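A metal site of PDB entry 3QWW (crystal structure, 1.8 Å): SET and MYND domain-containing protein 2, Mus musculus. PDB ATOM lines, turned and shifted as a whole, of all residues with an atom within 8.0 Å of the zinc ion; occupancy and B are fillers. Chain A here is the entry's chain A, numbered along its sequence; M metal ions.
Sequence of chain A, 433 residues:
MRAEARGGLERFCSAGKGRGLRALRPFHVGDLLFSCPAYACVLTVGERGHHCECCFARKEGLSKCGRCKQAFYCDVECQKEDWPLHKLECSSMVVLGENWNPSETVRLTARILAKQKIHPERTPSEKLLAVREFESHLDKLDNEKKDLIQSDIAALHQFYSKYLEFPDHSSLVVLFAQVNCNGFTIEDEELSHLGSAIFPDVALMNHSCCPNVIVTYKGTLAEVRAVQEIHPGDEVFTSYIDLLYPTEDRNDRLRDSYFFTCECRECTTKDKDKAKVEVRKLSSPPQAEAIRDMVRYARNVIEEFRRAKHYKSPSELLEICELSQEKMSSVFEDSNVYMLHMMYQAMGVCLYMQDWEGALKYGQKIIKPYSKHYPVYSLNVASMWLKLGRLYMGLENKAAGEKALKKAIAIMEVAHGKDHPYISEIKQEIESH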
ATOM      1  N   LYS A  64     -19.109 -16.008  24.827  1.00  0.00           N
ATOM      2  CA  LYS A  64     -18.501 -17.319  25.069  1.00  0.00           C
ATOM      3  C   LYS A  64     -17.955 -18.013  23.813  1.00  0.00           C
ATOM      4  O   LYS A  64     -18.386 -17.711  22.693  1.00  0.00           O
ATOM      5  CB  LYS A  64     -19.476 -18.237  25.841  1.00  0.00           C
ATOM      6  CG  LYS A  64     -20.659 -18.759  25.041  1.00  0.00           C
ATOM      7  CD  LYS A  64     -21.570 -19.653  25.874  1.00  0.00           C
ATOM      8  CE  LYS A  64     -22.720 -18.903  26.491  1.00  0.00           C
ATOM      9  NZ  LYS A  64     -23.639 -19.812  27.234  1.00  0.00           N
ATOM     10  N   CYS A  65     -17.025 -18.990  24.004  1.00  0.00           N
ATOM     11  CA  CYS A  65     -16.527 -19.791  22.894  1.00  0.00           C
ATOM     12  C   CYS A  65     -17.671 -20.693  22.424  1.00  0.00           C
ATOM     13  O   CYS A  65     -18.250 -21.422  23.241  1.00  0.00           O
ATOM     14  CB  CYS A  65     -15.320 -20.636  23.313  1.00  0.00           C
ATOM     15  SG  CYS A  65     -14.793 -21.797  22.046  1.00  0.00           S
ATOM     16  N   GLY A  66     -17.966 -20.648  21.130  1.00  0.00           N
ATOM     17  CA  GLY A  66     -19.030 -21.441  20.508  1.00  0.00           C
ATOM     18  C   GLY A  66     -18.947 -22.947  20.682  1.00  0.00           C
ATOM     19  O   GLY A  66     -19.981 -23.598  20.863  1.00  0.00           O
ATOM     20  N   ARG A  67     -17.718 -23.504  20.688  1.00  0.00           N
ATOM     21  CA  ARG A  67     -17.516 -24.949  20.819  1.00  0.00           C
ATOM     22  C   ARG A  67     -17.638 -25.510  22.221  1.00  0.00           C
ATOM     23  O   ARG A  67     -18.481 -26.387  22.443  1.00  0.00           O
ATOM     24  CB  ARG A  67     -16.248 -25.414  20.105  1.00  0.00           C
ATOM     25  CG  ARG A  67     -16.241 -26.908  19.804  1.00  0.00           C
ATOM     26  CD  ARG A  67     -15.327 -27.251  18.647  1.00  0.00           C
ATOM     27  NE  ARG A  67     -14.998 -28.679  18.620  1.00  0.00           N
ATOM     28  CZ  ARG A  67     -13.929 -29.214  19.189  1.00  0.00           C
ATOM     29  NH1 ARG A  67     -13.053 -28.443  19.830  1.00  0.00           N
ATOM     30  NH2 ARG A  67     -13.712 -30.520  19.117  1.00  0.00           N
ATOM     31  N   CYS A  68     -16.819 -25.033  23.166  1.00  0.00           N
ATOM     32  CA  CYS A  68     -16.824 -25.569  24.531  1.00  0.00           C
ATOM     33  C   CYS A  68     -17.801 -24.872  25.436  1.00  0.00           C
ATOM     34  O   CYS A  68     -18.147 -25.438  26.476  1.00  0.00           O
ATOM     35  CB  CYS A  68     -15.423 -25.531  25.118  1.00  0.00           C
ATOM     36  SG  CYS A  68     -14.719 -23.865  25.162  1.00  0.00           S
ATOM     37  N   LYS A  69     -18.200 -23.625  25.092  1.00  0.00           N
ATOM     38  CA  LYS A  69     -19.116 -22.788  25.895  1.00  0.00           C
ATOM     39  C   LYS A  69     -18.607 -22.590  27.332  1.00  0.00           C
ATOM     40  O   LYS A  69     -19.412 -22.377  28.247  1.00  0.00           O
ATOM     41  CB  LYS A  69     -20.569 -23.332  25.850  1.00  0.00           C
ATOM     42  CG  LYS A  69     -21.197 -23.215  24.451  1.00  0.00           C
ATOM     43  CD  LYS A  69     -22.662 -23.656  24.453  1.00  0.00           C
ATOM     44  CE  LYS A  69     -23.084 -24.221  23.115  1.00  0.00           C
ATOM     45  NZ  LYS A  69     -22.495 -25.570  22.865  1.00  0.00           N
ATOM     46  N   GLN A  70     -17.276 -22.637  27.528  1.00  0.00           N
ATOM     47  CA  GLN A  70     -16.608 -22.568  28.834  1.00  0.00           C
ATOM     48  C   GLN A  70     -15.678 -21.351  28.944  1.00  0.00           C
ATOM     49  O   GLN A  70     -15.580 -20.767  30.025  1.00  0.00           O
ATOM     50  CB  GLN A  70     -15.823 -23.867  29.074  1.00  0.00           C
ATOM     51  CG  GLN A  70     -15.461 -24.142  30.535  1.00  0.00           C
ATOM     52  CD  GLN A  70     -16.540 -24.895  31.276  1.00  0.00           C
ATOM     53  OE1 GLN A  70     -16.991 -25.963  30.860  1.00  0.00           O
ATOM     54  NE2 GLN A  70     -16.918 -24.377  32.445  1.00  0.00           N
ATOM     55  N   ALA A  71     -15.007 -20.980  27.843  1.00  0.00           N
ATOM     56  CA  ALA A  71     -14.107 -19.810  27.777  1.00  0.00           C
ATOM     57  C   ALA A  71     -14.943 -18.580  27.369  1.00  0.00           C
ATOM     58  O   ALA A  71     -15.714 -18.655  26.396  1.00  0.00           O
ATOM     59  CB  ALA A  71     -13.000 -20.053  26.761  1.00  0.00           C
ATOM     60  N   PHE A  72     -14.781 -17.465  28.124  1.00  0.00           N
ATOM     61  CA  PHE A  72     -15.510 -16.208  27.904  1.00  0.00           C
ATOM     62  C   PHE A  72     -14.560 -15.056  27.600  1.00  0.00           C
ATOM     63  O   PHE A  72     -13.450 -14.989  28.179  1.00  0.00           O
ATOM     64  CB  PHE A  72     -16.417 -15.874  29.091  1.00  0.00           C
ATOM     65  CG  PHE A  72     -17.542 -16.859  29.345  1.00  0.00           C
ATOM     66  CD1 PHE A  72     -17.295 -18.104  29.924  1.00  0.00           C
ATOM     67  CD2 PHE A  72     -18.867 -16.509  29.069  1.00  0.00           C
ATOM     68  CE1 PHE A  72     -18.348 -18.987  30.191  1.00  0.00           C
ATOM     69  CE2 PHE A  72     -19.911 -17.378  29.369  1.00  0.00           C
ATOM     70  CZ  PHE A  72     -19.647 -18.616  29.915  1.00  0.00           C
ATOM     71  N   TYR A  73     -14.970 -14.161  26.673  1.00  0.00           N
ATOM     72  CA  TYR A  73     -14.141 -13.077  26.158  1.00  0.00           C
ATOM     73  C   TYR A  73     -14.877 -11.741  25.990  1.00  0.00           C
ATOM     74  O   TYR A  73     -16.096 -11.728  25.784  1.00  0.00           O
ATOM     75  CB  TYR A  73     -13.526 -13.484  24.809  1.00  0.00           C
ATOM     76  CG  TYR A  73     -12.691 -14.755  24.841  1.00  0.00           C
ATOM     77  CD1 TYR A  73     -11.380 -14.748  25.300  1.00  0.00           C
ATOM     78  CD2 TYR A  73     -13.212 -15.965  24.371  1.00  0.00           C
ATOM     79  CE1 TYR A  73     -10.619 -15.918  25.321  1.00  0.00           C
ATOM     80  CE2 TYR A  73     -12.477 -17.146  24.427  1.00  0.00           C
ATOM     81  CZ  TYR A  73     -11.166 -17.110  24.867  1.00  0.00           C
ATOM     82  OH  TYR A  73     -10.404 -18.251  24.870  1.00  0.00           O
ATOM     83  N   GLN A  79     -10.713 -13.133  22.025  1.00  0.00           N
ATOM     84  CA  GLN A  79     -10.884 -14.557  21.661  1.00  0.00           C
ATOM     85  C   GLN A  79      -9.757 -15.030  20.734  1.00  0.00           C
ATOM     86  O   GLN A  79      -9.221 -16.136  20.901  1.00  0.00           O
ATOM     87  CB  GLN A  79     -12.259 -14.764  21.008  1.00  0.00           C
ATOM     88  CG  GLN A  79     -12.498 -16.174  20.510  1.00  0.00           C
ATOM     89  CD  GLN A  79     -13.909 -16.348  20.033  1.00  0.00           C
ATOM     90  OE1 GLN A  79     -14.506 -17.422  20.180  1.00  0.00           O
ATOM     91  NE2 GLN A  79     -14.484 -15.261  19.515  1.00  0.00           N
ATOM     92  N   TRP A  83      -6.789 -17.745  21.362  1.00  0.00           N
ATOM     93  CA  TRP A  83      -6.936 -18.980  20.578  1.00  0.00           C
ATOM     94  C   TRP A  83      -5.738 -19.940  20.569  1.00  0.00           C
ATOM     95  O   TRP A  83      -5.986 -21.120  20.840  1.00  0.00           O
ATOM     96  CB  TRP A  83      -7.538 -18.774  19.180  1.00  0.00           C
ATOM     97  CG  TRP A  83      -7.722 -20.055  18.421  1.00  0.00           C
ATOM     98  CD1 TRP A  83      -7.066 -20.424  17.285  1.00  0.00           C
ATOM     99  CD2 TRP A  83      -8.592 -21.152  18.748  1.00  0.00           C
ATOM    100  NE1 TRP A  83      -7.499 -21.664  16.865  1.00  0.00           N
ATOM    101  CE2 TRP A  83      -8.440 -22.133  17.739  1.00  0.00           C
ATOM    102  CE3 TRP A  83      -9.545 -21.386  19.772  1.00  0.00           C
ATOM    103  CZ2 TRP A  83      -9.154 -23.334  17.745  1.00  0.00           C
ATOM    104  CZ3 TRP A  83     -10.246 -22.584  19.782  1.00  0.00           C
ATOM    105  CH2 TRP A  83     -10.039 -23.546  18.781  1.00  0.00           C
ATOM    106  N   HIS A  86      -6.219 -21.349  24.179  1.00  0.00           N
ATOM    107  CA  HIS A  86      -7.505 -21.976  24.375  1.00  0.00           C
ATOM    108  C   HIS A  86      -7.684 -23.268  23.531  1.00  0.00           C
ATOM    109  O   HIS A  86      -8.349 -24.202  23.992  1.00  0.00           O
ATOM    110  CB  HIS A  86      -8.640 -20.981  24.080  1.00  0.00           C
ATOM    111  CG  HIS A  86      -9.963 -21.595  24.264  1.00  0.00           C
ATOM    112  ND1 HIS A  86     -10.375 -22.086  25.490  1.00  0.00           N
ATOM    113  CD2 HIS A  86     -10.925 -21.862  23.340  1.00  0.00           C
ATOM    114  CE1 HIS A  86     -11.572 -22.615  25.273  1.00  0.00           C
ATOM    115  NE2 HIS A  86     -11.934 -22.493  24.006  1.00  0.00           N
ATOM    116  N   LYS A  87      -7.081 -23.305  22.330  1.00  0.00           N
ATOM    117  CA  LYS A  87      -7.181 -24.477  21.428  1.00  0.00           C
ATOM    118  C   LYS A  87      -6.573 -25.754  22.033  1.00  0.00           C
ATOM    119  O   LYS A  87      -6.915 -26.861  21.620  1.00  0.00           O
ATOM    120  CB  LYS A  87      -6.592 -24.175  20.038  1.00  0.00           C
ATOM    121  CG  LYS A  87      -5.078 -24.108  19.935  1.00  0.00           C
ATOM    122  CD  LYS A  87      -4.658 -23.663  18.535  1.00  0.00           C
ATOM    123  CE  LYS A  87      -3.217 -23.996  18.278  1.00  0.00           C
ATOM    124  NZ  LYS A  87      -2.670 -23.290  17.094  1.00  0.00           N
ATOM    125  N   GLU A  89      -7.124 -26.628  25.081  1.00  0.00           N
ATOM    126  CA  GLU A  89      -8.049 -27.052  26.127  1.00  0.00           C
ATOM    127  C   GLU A  89      -9.490 -27.252  25.661  1.00  0.00           C
ATOM    128  O   GLU A  89     -10.229 -28.042  26.268  1.00  0.00           O
ATOM    129  CB  GLU A  89      -8.039 -26.028  27.273  1.00  0.00           C
ATOM    130  CG  GLU A  89      -6.632 -25.612  27.736  1.00  0.00           C
ATOM    131  CD  GLU A  89      -6.619 -24.685  28.933  1.00  0.00           C
ATOM    132  OE1 GLU A  89      -7.454 -23.751  28.982  1.00  0.00           O
ATOM    133  OE2 GLU A  89      -5.779 -24.887  29.833  1.00  0.00           O
ATOM    134  N   CYS A  90      -9.905 -26.464  24.649  1.00  0.00           N
ATOM    135  CA  CYS A  90     -11.250 -26.423  24.090  1.00  0.00           C
ATOM    136  C   CYS A  90     -11.862 -27.802  23.918  1.00  0.00           C
ATOM    137  O   CYS A  90     -12.805 -28.131  24.632  1.00  0.00           O
ATOM    138  CB  CYS A  90     -11.279 -25.640  22.786  1.00  0.00           C
ATOM    139  SG  CYS A  90     -12.966 -25.335  22.147  1.00  0.00           S
ATOM    140  N   SER A  91     -11.281 -28.618  23.025  1.00  0.00           N
ATOM    141  CA  SER A  91     -11.756 -29.968  22.701  1.00  0.00           C
ATOM    142  C   SER A  91     -11.798 -30.886  23.930  1.00  0.00           C
ATOM    143  O   SER A  91     -12.775 -31.603  24.103  1.00  0.00           O
ATOM    144  CB  SER A  91     -10.927 -30.572  21.582  1.00  0.00           C
ATOM    145  OG  SER A  91     -11.579 -31.708  21.022  1.00  0.00           O
ATOM    146  N   MET A  93     -12.191 -29.919  27.062  1.00  0.00           N
ATOM    147  CA  MET A  93     -13.262 -29.490  27.950  1.00  0.00           C
ATOM    148  C   MET A  93     -14.641 -29.978  27.437  1.00  0.00           C
ATOM    149  O   MET A  93     -15.555 -30.149  28.243  1.00  0.00           O
ATOM    150  CB  MET A  93     -13.249 -27.963  28.119  1.00  0.00           C
ATOM    151  CG  MET A  93     -12.121 -27.449  29.004  1.00  0.00           C
ATOM    152  SD  MET A  93     -12.158 -25.631  29.225  1.00  0.00           S
ATOM    153  CE  MET A  93     -11.710 -25.103  27.663  1.00  0.00           C
ATOM    154  N   VAL A  94     -14.773 -30.211  26.111  1.00  0.00           N
ATOM    155  CA  VAL A  94     -16.015 -30.721  25.495  1.00  0.00           C
ATOM    156  C   VAL A  94     -16.163 -32.207  25.834  1.00  0.00           C
ATOM    157  O   VAL A  94     -17.188 -32.601  26.398  1.00  0.00           O
ATOM    158  CB  VAL A  94     -16.070 -30.492  23.950  1.00  0.00           C
ATOM    159  CG1 VAL A  94     -17.419 -30.947  23.380  1.00  0.00           C
ATOM    160  CG2 VAL A  94     -15.796 -29.045  23.570  1.00  0.00           C
HETATM  161 ZN    ZN M   1     -13.649 -23.411  23.396  1.00  0.00          ZN
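The backbone NH of Gln 70 lies close to the side-chain sulfur of Cys 68. SG of Cys 65 lies close to N of Arg 67 (3.6 Å). The backbone NH (N) of Cys 65 lies within hydrogen-bond range of the backbone carbonyl oxygen (O) of Ala 71 (2.7 Å).
The zinc ion is bound by a ring nitrogen (NE2) of His 86 (2.0 Å), the side-chain sulfur (SG) of Cys 68 (2.1 Å), the side-chain sulfur (SG) of Cys 90 (2.4 Å) and the side-chain sulfur (SG) of Cys 65 (2.4 Å). The zinc ion has four donor atoms within binding distance.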
